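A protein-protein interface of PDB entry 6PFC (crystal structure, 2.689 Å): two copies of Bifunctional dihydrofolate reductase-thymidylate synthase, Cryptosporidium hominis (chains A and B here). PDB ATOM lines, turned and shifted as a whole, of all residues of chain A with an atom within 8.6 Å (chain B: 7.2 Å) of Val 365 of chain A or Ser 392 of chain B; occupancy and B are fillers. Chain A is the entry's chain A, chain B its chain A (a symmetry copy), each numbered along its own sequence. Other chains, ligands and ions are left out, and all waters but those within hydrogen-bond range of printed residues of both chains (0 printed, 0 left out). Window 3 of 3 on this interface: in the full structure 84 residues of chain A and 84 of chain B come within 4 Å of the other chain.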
ATOM      1  N   GLY A 343      29.150  -1.805  23.974  1.00  0.00           N
ATOM      2  CA  GLY A 343      30.456  -2.159  23.465  1.00  0.00           C
ATOM      3  C   GLY A 343      30.951  -3.534  23.847  1.00  0.00           C
ATOM      4  O   GLY A 343      31.921  -4.013  23.246  1.00  0.00           O
ATOM      5  N   PHE A 344      30.279  -4.231  24.755  1.00  0.00           N
ATOM      6  CA  PHE A 344      30.599  -5.632  24.981  1.00  0.00           C
ATOM      7  C   PHE A 344      29.552  -6.537  24.372  1.00  0.00           C
ATOM      8  O   PHE A 344      29.883  -7.628  23.910  1.00  0.00           O
ATOM      9  CB  PHE A 344      30.725  -5.945  26.479  1.00  0.00           C
ATOM     10  CG  PHE A 344      31.213  -7.347  26.773  1.00  0.00           C
ATOM     11  CD1 PHE A 344      30.330  -8.407  26.892  1.00  0.00           C
ATOM     12  CD2 PHE A 344      32.570  -7.597  26.915  1.00  0.00           C
ATOM     13  CE1 PHE A 344      30.788  -9.693  27.153  1.00  0.00           C
ATOM     14  CE2 PHE A 344      33.033  -8.880  27.177  1.00  0.00           C
ATOM     15  CZ  PHE A 344      32.141  -9.927  27.296  1.00  0.00           C
ATOM     16  N   GLN A 345      28.299  -6.087  24.341  1.00  0.00           N
ATOM     17  CA  GLN A 345      27.291  -6.729  23.514  1.00  0.00           C
ATOM     18  C   GLN A 345      27.438  -6.342  22.047  1.00  0.00           C
ATOM     19  O   GLN A 345      26.985  -7.088  21.172  1.00  0.00           O
ATOM     20  CB  GLN A 345      25.892  -6.367  24.016  1.00  0.00           C
ATOM     21  CG  GLN A 345      25.691  -6.578  25.512  1.00  0.00           C
ATOM     22  CD  GLN A 345      25.923  -8.013  25.950  1.00  0.00           C
ATOM     23  OE1 GLN A 345      25.636  -8.957  25.211  1.00  0.00           O
ATOM     24  NE2 GLN A 345      26.451  -8.184  27.157  1.00  0.00           N
ATOM     25  N   TRP A 346      28.059  -5.190  21.768  1.00  0.00           N
ATOM     26  CA  TRP A 346      28.284  -4.776  20.385  1.00  0.00           C
ATOM     27  C   TRP A 346      29.342  -5.637  19.706  1.00  0.00           C
ATOM     28  O   TRP A 346      29.189  -6.011  18.537  1.00  0.00           O
ATOM     29  CB  TRP A 346      28.699  -3.306  20.337  1.00  0.00           C
ATOM     30  CG  TRP A 346      27.622  -2.327  20.705  1.00  0.00           C
ATOM     31  CD1 TRP A 346      26.428  -2.599  21.311  1.00  0.00           C
ATOM     32  CD2 TRP A 346      27.642  -0.913  20.477  1.00  0.00           C
ATOM     33  NE1 TRP A 346      25.708  -1.441  21.480  1.00  0.00           N
ATOM     34  CE2 TRP A 346      26.431  -0.392  20.976  1.00  0.00           C
ATOM     35  CE3 TRP A 346      28.568  -0.037  19.902  1.00  0.00           C
ATOM     36  CZ2 TRP A 346      26.123   0.966  20.916  1.00  0.00           C
ATOM     37  CZ3 TRP A 346      28.259   1.310  19.843  1.00  0.00           C
ATOM     38  CH2 TRP A 346      27.048   1.799  20.346  1.00  0.00           C
ATOM     39  N   ARG A 347      30.425  -5.957  20.415  1.00  0.00           N
ATOM     40  CA  ARG A 347      31.566  -6.645  19.824  1.00  0.00           C
ATOM     41  C   ARG A 347      31.712  -8.094  20.259  1.00  0.00           C
ATOM     42  O   ARG A 347      32.308  -8.885  19.525  1.00  0.00           O
ATOM     43  CB  ARG A 347      32.865  -5.900  20.156  1.00  0.00           C
ATOM     44  CG  ARG A 347      32.813  -4.403  19.895  1.00  0.00           C
ATOM     45  CD  ARG A 347      32.410  -4.102  18.463  1.00  0.00           C
ATOM     46  NE  ARG A 347      33.282  -4.769  17.502  1.00  0.00           N
ATOM     47  CZ  ARG A 347      34.436  -4.269  17.070  1.00  0.00           C
ATOM     48  NH1 ARG A 347      34.860  -3.095  17.516  1.00  0.00           N
ATOM     49  NH2 ARG A 347      35.165  -4.946  16.193  1.00  0.00           N
ATOM     50  N   HIS A 348      31.197  -8.463  21.434  1.00  0.00           N
ATOM     51  CA  HIS A 348      31.333  -9.817  21.961  1.00  0.00           C
ATOM     52  C   HIS A 348      30.005 -10.254  22.585  1.00  0.00           C
ATOM     53  O   HIS A 348      29.914 -10.569  23.769  1.00  0.00           O
ATOM     54  CB  HIS A 348      32.471  -9.898  22.978  1.00  0.00           C
ATOM     55  CG  HIS A 348      33.692  -9.124  22.585  1.00  0.00           C
ATOM     56  ND1 HIS A 348      34.542  -9.531  21.580  1.00  0.00           N
ATOM     57  CD2 HIS A 348      34.204  -7.967  23.067  1.00  0.00           C
ATOM     58  CE1 HIS A 348      35.524  -8.656  21.457  1.00  0.00           C
ATOM     59  NE2 HIS A 348      35.344  -7.699  22.348  1.00  0.00           N
ATOM     60  N   TYR A 349      28.950 -10.262  21.774  1.00  0.00           N
ATOM     61  CA  TYR A 349      27.626 -10.612  22.273  1.00  0.00           C
ATOM     62  C   TYR A 349      27.584 -12.069  22.720  1.00  0.00           C
ATOM     63  O   TYR A 349      28.137 -12.953  22.060  1.00  0.00           O
ATOM     64  CB  TYR A 349      26.568 -10.361  21.198  1.00  0.00           C
ATOM     65  CG  TYR A 349      25.149 -10.455  21.710  1.00  0.00           C
ATOM     66  CD1 TYR A 349      24.493  -9.334  22.203  1.00  0.00           C
ATOM     67  CD2 TYR A 349      24.465 -11.665  21.706  1.00  0.00           C
ATOM     68  CE1 TYR A 349      23.197  -9.414  22.676  1.00  0.00           C
ATOM     69  CE2 TYR A 349      23.171 -11.754  22.179  1.00  0.00           C
ATOM     70  CZ  TYR A 349      22.541 -10.626  22.660  1.00  0.00           C
ATOM     71  OH  TYR A 349      21.250 -10.712  23.130  1.00  0.00           O
ATOM     72  N   ASN A 350      26.917 -12.308  23.852  1.00  0.00           N
ATOM     73  CA  ASN A 350      26.802 -13.629  24.471  1.00  0.00           C
ATOM     74  C   ASN A 350      28.156 -14.208  24.868  1.00  0.00           C
ATOM     75  O   ASN A 350      28.300 -15.429  24.991  1.00  0.00           O
ATOM     76  CB  ASN A 350      26.055 -14.614  23.563  1.00  0.00           C
ATOM     77  CG  ASN A 350      24.554 -14.496  23.694  1.00  0.00           C
ATOM     78  OD1 ASN A 350      24.042 -14.083  24.734  1.00  0.00           O
ATOM     79  ND2 ASN A 350      23.837 -14.859  22.639  1.00  0.00           N
ATOM     80  N   GLY A 351      29.158 -13.356  25.069  1.00  0.00           N
ATOM     81  CA  GLY A 351      30.465 -13.808  25.506  1.00  0.00           C
ATOM     82  C   GLY A 351      30.539 -13.880  27.023  1.00  0.00           C
ATOM     83  O   GLY A 351      30.037 -13.006  27.726  1.00  0.00           O
ATOM     84  N   GLU A 352      31.173 -14.942  27.516  1.00  0.00           N
ATOM     85  CA  GLU A 352      31.315 -15.145  28.955  1.00  0.00           C
ATOM     86  C   GLU A 352      32.224 -14.062  29.527  1.00  0.00           C
ATOM     87  O   GLU A 352      33.421 -14.022  29.224  1.00  0.00           O
ATOM     88  CB  GLU A 352      31.872 -16.537  29.241  1.00  0.00           C
ATOM     89  N   TYR A 360      39.123 -10.522  25.125  1.00  0.00           N
ATOM     90  CA  TYR A 360      37.894 -11.073  24.569  1.00  0.00           C
ATOM     91  C   TYR A 360      37.901 -11.090  23.043  1.00  0.00           C
ATOM     92  O   TYR A 360      36.841 -11.217  22.423  1.00  0.00           O
ATOM     93  CB  TYR A 360      36.682 -10.295  25.081  1.00  0.00           C
ATOM     94  CG  TYR A 360      36.492 -10.364  26.579  1.00  0.00           C
ATOM     95  CD1 TYR A 360      35.862 -11.451  27.169  1.00  0.00           C
ATOM     96  CD2 TYR A 360      36.936  -9.337  27.403  1.00  0.00           C
ATOM     97  CE1 TYR A 360      35.682 -11.517  28.538  1.00  0.00           C
ATOM     98  CE2 TYR A 360      36.761  -9.394  28.772  1.00  0.00           C
ATOM     99  CZ  TYR A 360      36.133 -10.485  29.334  1.00  0.00           C
ATOM    100  OH  TYR A 360      35.957 -10.546  30.699  1.00  0.00           O
ATOM    101  N   GLY A 362      37.744 -12.487  19.716  1.00  0.00           N
ATOM    102  CA  GLY A 362      37.328 -13.727  19.093  1.00  0.00           C
ATOM    103  C   GLY A 362      36.097 -14.354  19.721  1.00  0.00           C
ATOM    104  O   GLY A 362      35.366 -15.082  19.036  1.00  0.00           O
ATOM    105  N   VAL A 363      35.847 -14.084  21.003  1.00  0.00           N
ATOM    106  CA  VAL A 363      34.713 -14.665  21.715  1.00  0.00           C
ATOM    107  C   VAL A 363      33.487 -13.788  21.501  1.00  0.00           C
ATOM    108  O   VAL A 363      33.589 -12.558  21.416  1.00  0.00           O
ATOM    109  CB  VAL A 363      35.029 -14.840  23.215  1.00  0.00           C
ATOM    110  CG1 VAL A 363      35.187 -13.493  23.903  1.00  0.00           C
ATOM    111  CG2 VAL A 363      33.953 -15.675  23.899  1.00  0.00           C
ATOM    112  N   GLY A 364      32.324 -14.423  21.397  1.00  0.00           N
ATOM    113  CA  GLY A 364      31.077 -13.709  21.228  1.00  0.00           C
ATOM    114  C   GLY A 364      30.828 -13.299  19.789  1.00  0.00           C
ATOM    115  O   GLY A 364      31.679 -13.428  18.906  1.00  0.00           O
ATOM    116  N   VAL A 365      29.620 -12.799  19.551  1.00  0.00           N
ATOM    117  CA  VAL A 365      29.213 -12.340  18.228  1.00  0.00           C
ATOM    118  C   VAL A 365      29.569 -10.867  18.086  1.00  0.00           C
ATOM    119  O   VAL A 365      29.187 -10.042  18.925  1.00  0.00           O
ATOM    120  CB  VAL A 365      27.709 -12.569  18.003  1.00  0.00           C
ATOM    121  CG1 VAL A 365      27.292 -12.057  16.632  1.00  0.00           C
ATOM    122  CG2 VAL A 365      27.368 -14.043  18.154  1.00  0.00           C
ATOM    123  N   ASP A 366      30.307 -10.539  17.026  1.00  0.00           N
ATOM    124  CA  ASP A 366      30.696  -9.159  16.736  1.00  0.00           C
ATOM    125  C   ASP A 366      29.616  -8.545  15.854  1.00  0.00           C
ATOM    126  O   ASP A 366      29.665  -8.628  14.626  1.00  0.00           O
ATOM    127  CB  ASP A 366      32.068  -9.113  16.073  1.00  0.00           C
ATOM    128  CG  ASP A 366      32.709  -7.738  16.148  1.00  0.00           C
ATOM    129  OD1 ASP A 366      31.971  -6.732  16.221  1.00  0.00           O
ATOM    130  OD2 ASP A 366      33.955  -7.665  16.130  1.00  0.00           O
ATOM    131  N   GLN A 367      28.620  -7.926  16.492  1.00  0.00           N
ATOM    132  CA  GLN A 367      27.526  -7.323  15.736  1.00  0.00           C
ATOM    133  C   GLN A 367      28.015  -6.169  14.872  1.00  0.00           C
ATOM    134  O   GLN A 367      27.609  -6.040  13.710  1.00  0.00           O
ATOM    135  CB  GLN A 367      26.426  -6.844  16.681  1.00  0.00           C
ATOM    136  CG  GLN A 367      25.681  -7.951  17.393  1.00  0.00           C
ATOM    137  CD  GLN A 367      24.498  -7.424  18.168  1.00  0.00           C
ATOM    138  OE1 GLN A 367      23.421  -7.217  17.609  1.00  0.00           O
ATOM    139  NE2 GLN A 367      24.690  -7.198  19.463  1.00  0.00           N
ATOM    140  N   LEU A 368      28.885  -5.318  15.421  1.00  0.00           N
ATOM    141  CA  LEU A 368      29.329  -4.137  14.688  1.00  0.00           C
ATOM    142  C   LEU A 368      30.076  -4.522  13.418  1.00  0.00           C
ATOM    143  O   LEU A 368      29.907  -3.882  12.373  1.00  0.00           O
ATOM    144  CB  LEU A 368      30.202  -3.263  15.586  1.00  0.00           C
ATOM    145  CG  LEU A 368      30.623  -1.912  15.001  1.00  0.00           C
ATOM    146  CD1 LEU A 368      29.407  -1.095  14.586  1.00  0.00           C
ATOM    147  CD2 LEU A 368      31.472  -1.146  16.001  1.00  0.00           C
ATOM    148  N   ALA A 369      30.911  -5.560  13.486  1.00  0.00           N
ATOM    149  CA  ALA A 369      31.621  -6.016  12.296  1.00  0.00           C
ATOM    150  C   ALA A 369      30.650  -6.557  11.254  1.00  0.00           C
ATOM    151  O   ALA A 369      30.726  -6.201  10.072  1.00  0.00           O
ATOM    152  CB  ALA A 369      32.657  -7.075  12.674  1.00  0.00           C
ATOM    153  N   LYS A 370      29.721  -7.419  11.678  1.00  0.00           N
ATOM    154  CA  LYS A 370      28.734  -7.959  10.749  1.00  0.00           C
ATOM    155  C   LYS A 370      27.780  -6.882  10.250  1.00  0.00           C
ATOM    156  O   LYS A 370      27.280  -6.974   9.123  1.00  0.00           O
ATOM    157  CB  LYS A 370      27.950  -9.094  11.411  1.00  0.00           C
ATOM    158  CG  LYS A 370      28.822 -10.219  11.943  1.00  0.00           C
ATOM    159  CD  LYS A 370      27.986 -11.372  12.478  1.00  0.00           C
ATOM    160  CE  LYS A 370      27.273 -12.107  11.355  1.00  0.00           C
ATOM    161  NZ  LYS A 370      26.541 -13.304  11.851  1.00  0.00           N
ATOM    162  N   LEU A 371      27.516  -5.860  11.068  1.00  0.00           N
ATOM    163  CA  LEU A 371      26.673  -4.755  10.624  1.00  0.00           C
ATOM    164  C   LEU A 371      27.328  -3.997   9.478  1.00  0.00           C
ATOM    165  O   LEU A 371      26.703  -3.755   8.438  1.00  0.00           O
ATOM    166  CB  LEU A 371      26.380  -3.817  11.796  1.00  0.00           C
ATOM    167  CG  LEU A 371      25.689  -2.494  11.457  1.00  0.00           C
ATOM    168  CD1 LEU A 371      24.301  -2.744  10.887  1.00  0.00           C
ATOM    169  CD2 LEU A 371      25.620  -1.587  12.679  1.00  0.00           C
ATOM    170  N   LEU A 386      21.532  -3.482  15.526  1.00  0.00           N
ATOM    171  CA  LEU A 386      22.513  -3.567  16.601  1.00  0.00           C
ATOM    172  C   LEU A 386      21.765  -3.513  17.926  1.00  0.00           C
ATOM    173  O   LEU A 386      21.087  -2.522  18.217  1.00  0.00           O
ATOM    174  CB  LEU A 386      23.533  -2.431  16.508  1.00  0.00           C
ATOM    175  CG  LEU A 386      24.482  -2.272  17.697  1.00  0.00           C
ATOM    176  CD1 LEU A 386      25.393  -3.482  17.823  1.00  0.00           C
ATOM    177  CD2 LEU A 386      25.294  -0.990  17.574  1.00  0.00           C
ATOM    178  N   THR A 387      21.879  -4.576  18.720  1.00  0.00           N
ATOM    179  CA  THR A 387      21.170  -4.680  19.987  1.00  0.00           C
ATOM    180  C   THR A 387      22.153  -4.782  21.145  1.00  0.00           C
ATOM    181  O   THR A 387      23.288  -5.241  20.984  1.00  0.00           O
ATOM    182  CB  THR A 387      20.227  -5.892  20.019  1.00  0.00           C
ATOM    183  OG1 THR A 387      19.535  -5.920  21.273  1.00  0.00           O
ATOM    184  CG2 THR A 387      21.007  -7.186  19.855  1.00  0.00           C
ATOM    185  N   ASN A 390      20.727  -8.000  26.523  1.00  0.00           N
ATOM    186  CA  ASN A 390      21.019  -9.420  26.693  1.00  0.00           C
ATOM    187  C   ASN A 390      20.472  -9.874  28.038  1.00  0.00           C
ATOM    188  O   ASN A 390      21.080  -9.589  29.082  1.00  0.00           O
ATOM    189  CB  ASN A 390      22.527  -9.677  26.606  1.00  0.00           C
ATOM    190  CG  ASN A 390      22.861 -11.144  26.408  1.00  0.00           C
ATOM    191  OD1 ASN A 390      22.138 -12.029  26.866  1.00  0.00           O
ATOM    192  ND2 ASN A 390      23.966 -11.409  25.721  1.00  0.00           N
ATOM    193  N   GLN B 345      12.623 -17.481  22.300  1.00  0.00           N
ATOM    194  CA  GLN B 345      13.352 -16.431  22.992  1.00  0.00           C
ATOM    195  C   GLN B 345      12.534 -15.837  24.133  1.00  0.00           C
ATOM    196  O   GLN B 345      13.114 -15.276  25.069  1.00  0.00           O
ATOM    197  CB  GLN B 345      13.753 -15.333  22.005  1.00  0.00           C
ATOM    198  CG  GLN B 345      14.448 -15.845  20.748  1.00  0.00           C
ATOM    199  CD  GLN B 345      15.723 -16.615  21.043  1.00  0.00           C
ATOM    200  OE1 GLN B 345      16.446 -16.308  21.993  1.00  0.00           O
ATOM    201  NE2 GLN B 345      16.003 -17.626  20.229  1.00  0.00           N
ATOM    202  N   TYR B 349      15.238 -18.082  26.453  1.00  0.00           N
ATOM    203  CA  TYR B 349      16.223 -17.239  25.790  1.00  0.00           C
ATOM    204  C   TYR B 349      17.632 -17.781  26.007  1.00  0.00           C
ATOM    205  O   TYR B 349      17.983 -18.219  27.106  1.00  0.00           O
ATOM    206  CB  TYR B 349      16.128 -15.802  26.305  1.00  0.00           C
ATOM    207  CG  TYR B 349      16.936 -14.813  25.496  1.00  0.00           C
ATOM    208  CD1 TYR B 349      16.373 -14.152  24.411  1.00  0.00           C
ATOM    209  CD2 TYR B 349      18.261 -14.543  25.812  1.00  0.00           C
ATOM    210  CE1 TYR B 349      17.106 -13.249  23.665  1.00  0.00           C
ATOM    211  CE2 TYR B 349      19.002 -13.644  25.070  1.00  0.00           C
ATOM    212  CZ  TYR B 349      18.420 -12.999  24.000  1.00  0.00           C
ATOM    213  OH  TYR B 349      19.155 -12.101  23.261  1.00  0.00           O
ATOM    214  N   ASN B 350      18.437 -17.743  24.942  1.00  0.00           N
ATOM    215  CA  ASN B 350      19.807 -18.258  24.932  1.00  0.00           C
ATOM    216  C   ASN B 350      19.871 -19.754  25.224  1.00  0.00           C
ATOM    217  O   ASN B 350      20.906 -20.257  25.674  1.00  0.00           O
ATOM    218  CB  ASN B 350      20.703 -17.492  25.912  1.00  0.00           C
ATOM    219  CG  ASN B 350      21.251 -16.214  25.319  1.00  0.00           C
ATOM    220  OD1 ASN B 350      21.401 -16.099  24.103  1.00  0.00           O
ATOM    221  ND2 ASN B 350      21.554 -15.246  26.173  1.00  0.00           N
ATOM    222  N   TRP B 389      15.311 -10.590  19.646  1.00  0.00           N
ATOM    223  CA  TRP B 389      16.461 -10.495  18.749  1.00  0.00           C
ATOM    224  C   TRP B 389      17.669 -11.118  19.434  1.00  0.00           C
ATOM    225  O   TRP B 389      18.296 -10.500  20.299  1.00  0.00           O
ATOM    226  CB  TRP B 389      16.727  -9.045  18.364  1.00  0.00           C
ATOM    227  CG  TRP B 389      17.703  -8.899  17.240  1.00  0.00           C
ATOM    228  CD1 TRP B 389      19.031  -8.607  17.343  1.00  0.00           C
ATOM    229  CD2 TRP B 389      17.430  -9.042  15.842  1.00  0.00           C
ATOM    230  NE1 TRP B 389      19.604  -8.559  16.095  1.00  0.00           N
ATOM    231  CE2 TRP B 389      18.642  -8.822  15.156  1.00  0.00           C
ATOM    232  CE3 TRP B 389      16.280  -9.333  15.102  1.00  0.00           C
ATOM    233  CZ2 TRP B 389      18.736  -8.884  13.767  1.00  0.00           C
ATOM    234  CZ3 TRP B 389      16.376  -9.396  13.721  1.00  0.00           C
ATOM    235  CH2 TRP B 389      17.595  -9.172  13.069  1.00  0.00           C
ATOM    236  N   ASN B 390      17.995 -12.349  19.050  1.00  0.00           N
ATOM    237  CA  ASN B 390      19.154 -13.054  19.585  1.00  0.00           C
ATOM    238  C   ASN B 390      20.159 -13.268  18.462  1.00  0.00           C
ATOM    239  O   ASN B 390      19.964 -14.157  17.618  1.00  0.00           O
ATOM    240  CB  ASN B 390      18.738 -14.394  20.202  1.00  0.00           C
ATOM    241  CG  ASN B 390      19.816 -14.992  21.085  1.00  0.00           C
ATOM    242  OD1 ASN B 390      21.010 -14.795  20.857  1.00  0.00           O
ATOM    243  ND2 ASN B 390      19.398 -15.732  22.106  1.00  0.00           N
ATOM    244  N   PRO B 391      21.236 -12.480  18.394  1.00  0.00           N
ATOM    245  CA  PRO B 391      22.209 -12.654  17.302  1.00  0.00           C
ATOM    246  C   PRO B 391      22.851 -14.029  17.262  1.00  0.00           C
ATOM    247  O   PRO B 391      23.329 -14.440  16.197  1.00  0.00           O
ATOM    248  CB  PRO B 391      23.251 -11.563  17.585  1.00  0.00           C
ATOM    249  CG  PRO B 391      22.512 -10.533  18.374  1.00  0.00           C
ATOM    250  CD  PRO B 391      21.527 -11.293  19.216  1.00  0.00           C
ATOM    251  N   SER B 392      22.873 -14.758  18.379  1.00  0.00           N
ATOM    252  CA  SER B 392      23.483 -16.082  18.400  1.00  0.00           C
ATOM    253  C   SER B 392      22.591 -17.152  17.788  1.00  0.00           C
ATOM    254  O   SER B 392      23.081 -18.241  17.473  1.00  0.00           O
ATOM    255  CB  SER B 392      23.833 -16.480  19.835  1.00  0.00           C
ATOM    256  OG  SER B 392      24.739 -15.559  20.418  1.00  0.00           O
ATOM    257  N   ALA B 393      21.302 -16.868  17.604  1.00  0.00           N
ATOM    258  CA  ALA B 393      20.359 -17.856  17.104  1.00  0.00           C
ATOM    259  C   ALA B 393      19.747 -17.487  15.761  1.00  0.00           C
ATOM    260  O   ALA B 393      18.946 -18.267  15.232  1.00  0.00           O
ATOM    261  CB  ALA B 393      19.238 -18.083  18.129  1.00  0.00           C
ATOM    262  N   LEU B 394      20.097 -16.326  15.197  1.00  0.00           N
ATOM    263  CA  LEU B 394      19.478 -15.882  13.949  1.00  0.00           C
ATOM    264  C   LEU B 394      19.708 -16.880  12.820  1.00  0.00           C
ATOM    265  O   LEU B 394      18.820 -17.099  11.986  1.00  0.00           O
ATOM    266  CB  LEU B 394      20.015 -14.505  13.556  1.00  0.00           C
ATOM    267  CG  LEU B 394      19.694 -13.349  14.503  1.00  0.00           C
ATOM    268  CD1 LEU B 394      20.360 -12.069  14.030  1.00  0.00           C
ATOM    269  CD2 LEU B 394      18.191 -13.161  14.622  1.00  0.00           C
ATOM    270  N   SER B 395      20.892 -17.495  12.776  1.00  0.00           N
ATOM    271  CA  SER B 395      21.204 -18.420  11.691  1.00  0.00           C
ATOM    272  C   SER B 395      20.326 -19.665  11.737  1.00  0.00           C
ATOM    273  O   SER B 395      20.095 -20.296  10.699  1.00  0.00           O
ATOM    274  CB  SER B 395      22.681 -18.808  11.745  1.00  0.00           C
ATOM    275  OG  SER B 395      23.022 -19.335  13.015  1.00  0.00           O
ATOM    276  N   GLN B 396      19.833 -20.033  12.920  1.00  0.00           N
ATOM    277  CA  GLN B 396      18.966 -21.192  13.079  1.00  0.00           C
ATOM    278  C   GLN B 396      17.495 -20.876  12.841  1.00  0.00           C
ATOM    279  O   GLN B 396      16.682 -21.804  12.768  1.00  0.00           O
ATOM    280  CB  GLN B 396      19.136 -21.793  14.480  1.00  0.00           C
ATOM    281  CG  GLN B 396      20.534 -22.319  14.770  1.00  0.00           C
ATOM    282  CD  GLN B 396      20.672 -22.881  16.173  1.00  0.00           C
ATOM    283  OE1 GLN B 396      20.150 -22.318  17.136  1.00  0.00           O
ATOM    284  NE2 GLN B 396      21.374 -24.002  16.296  1.00  0.00           N
ATOM    285  N   MET B 397      17.136 -19.601  12.712  1.00  0.00           N
ATOM    286  CA  MET B 397      15.741 -19.215  12.568  1.00  0.00           C
ATOM    287  C   MET B 397      15.283 -19.320  11.119  1.00  0.00           C
ATOM    288  O   MET B 397      16.021 -18.978  10.190  1.00  0.00           O
ATOM    289  CB  MET B 397      15.526 -17.787  13.067  1.00  0.00           C
ATOM    290  CG  MET B 397      15.881 -17.592  14.520  1.00  0.00           C
ATOM    291  SD  MET B 397      15.541 -15.936  15.145  1.00  0.00           S
ATOM    292  CE  MET B 397      16.246 -16.050  16.790  1.00  0.00           C
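The side-chain hydroxyl of Tyr 349 of chain B sits at hydrogen-bond distance from the side-chain hydroxyl of Tyr 349 of chain A. OD1 of Asn 390 of chain A is in hydrogen-bond range of ND2 of Asn 350 of chain B (3.3 Å). The side-chain amide nitrogen (ND2) of Asn 350 of chain A lies within hydrogen-bond range of the side-chain amide oxygen (OD1) of Asn 390 of chain B (3.3 Å). The side-chain amide nitrogen of Asn 350 of chain B sits at hydrogen-bond distance from the side-chain amide oxygen of Asn 350 of chain A, 3.1 Å away. The side-chain hydroxyl (OG) of Ser 392 of chain B sits at hydrogen-bond distance from the side-chain amide nitrogen (ND2) of Asn 350 of chain A.
The side-chain amide nitrogen of Asn 390 of chain A sits at hydrogen-bond distance from the side-chain amide oxygen of Gln 345 of chain A (3.0 Å). OH of Tyr 349 of chain B is in hydrogen-bond range of O of Trp 389 of chain B (3.5 Å). The side-chain amide nitrogen of Gln 367 of chain A sits at hydrogen-bond distance from the backbone carbonyl oxygen of Thr 387 of chain A (2.8 Å). The backbone carbonyl oxygen of Val 365 of chain A lies within hydrogen-bond range of the backbone NH of Tyr 349 of chain A, at 2.9 Å. The side-chain amide oxygen (OD1) of Asn 390 of chain B sits close to the backbone NH (N) of Ser 392 of chain B (3.1 Å). The side-chain amide oxygen (OD1) of Asn 350 of chain B lies within hydrogen-bond range of the side-chain amide nitrogen (ND2) of Asn 390 of chain B.
Tyr 349 of chain A touches Asn 390 of chain B (CE2 to OD1, 3.96 Å). Pro 391 of chain B touches Tyr 349 of chain A. Val 365 of chain A touches Ser 392 of chain B (CG2 to OG, 3.8 Å). Pro 391 of chain B touches Gln 367 of chain A. Thr 387 of chain A touches Trp 389 of chain B. Pro 391 of chain B touches Thr 387 of chain A (CG to CG2, 3.96 Å). Tyr 349 of chain B touches Asn 390 of chain A (CE2 to OD1, 3.96 Å).
Of chain B, only Ser 392 comes within 4 Å of Val 365 of chain A. Of the printed residues of chain B, Thr 387 of chain A touches Trp 389 and Pro 391. Of the printed residues of chain B, Asn 390 of chain A touches Tyr 349 (3.96 Å) and Asn 350 (3.3 Å). Pro 391 of chain B touches just these residues of chain A: Tyr 349, Gln 367 and Thr 387. Ser 392 of chain B touches two residues of chain A. Ala 393 of chain B touches none of the printed residues of chain A. Gln 396 of chain B touches none of the printed residues of chain A. The nearest residue of chain B that does not touch Val 365 of chain A is Pro 391 of chain B (4.2 Å).
Hydrophobic or aromatic side chains of chain B within 4 Å of the printed part of chain A: Tyr 349, Trp 389 and Pro 391. Printed residues of chain A that touch a printed residue of chain B: Tyr 349, Asn 350, Val 365, Gln 367, Thr 387 and Asn 390. Hydrophobic or aromatic side chains of chain A that line the printed part of chain B: Tyr 349 and Val 365. Among the printed residues, 12 pairs touch across the chains. Among the printed residues, no Asp or Glu carboxylate lies within 4 Å of a Lys or Arg side-chain nitrogen of the other chain.
Tyr 349 of chain A touches its own counterpart, Tyr 349 of chain B. Tyr 349 of chain A touches Asn 390 of chain B, and with the chains exchanged Asn 390 of chain A touches Tyr 349 of chain B. Asn 350 of chain B touches its own counterpart, Asn 350 of chain A. Asn 350 of chain A touches Asn 390 of chain B, and with the chains exchanged Asn 390 of chain A touches Asn 350 of chain B.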
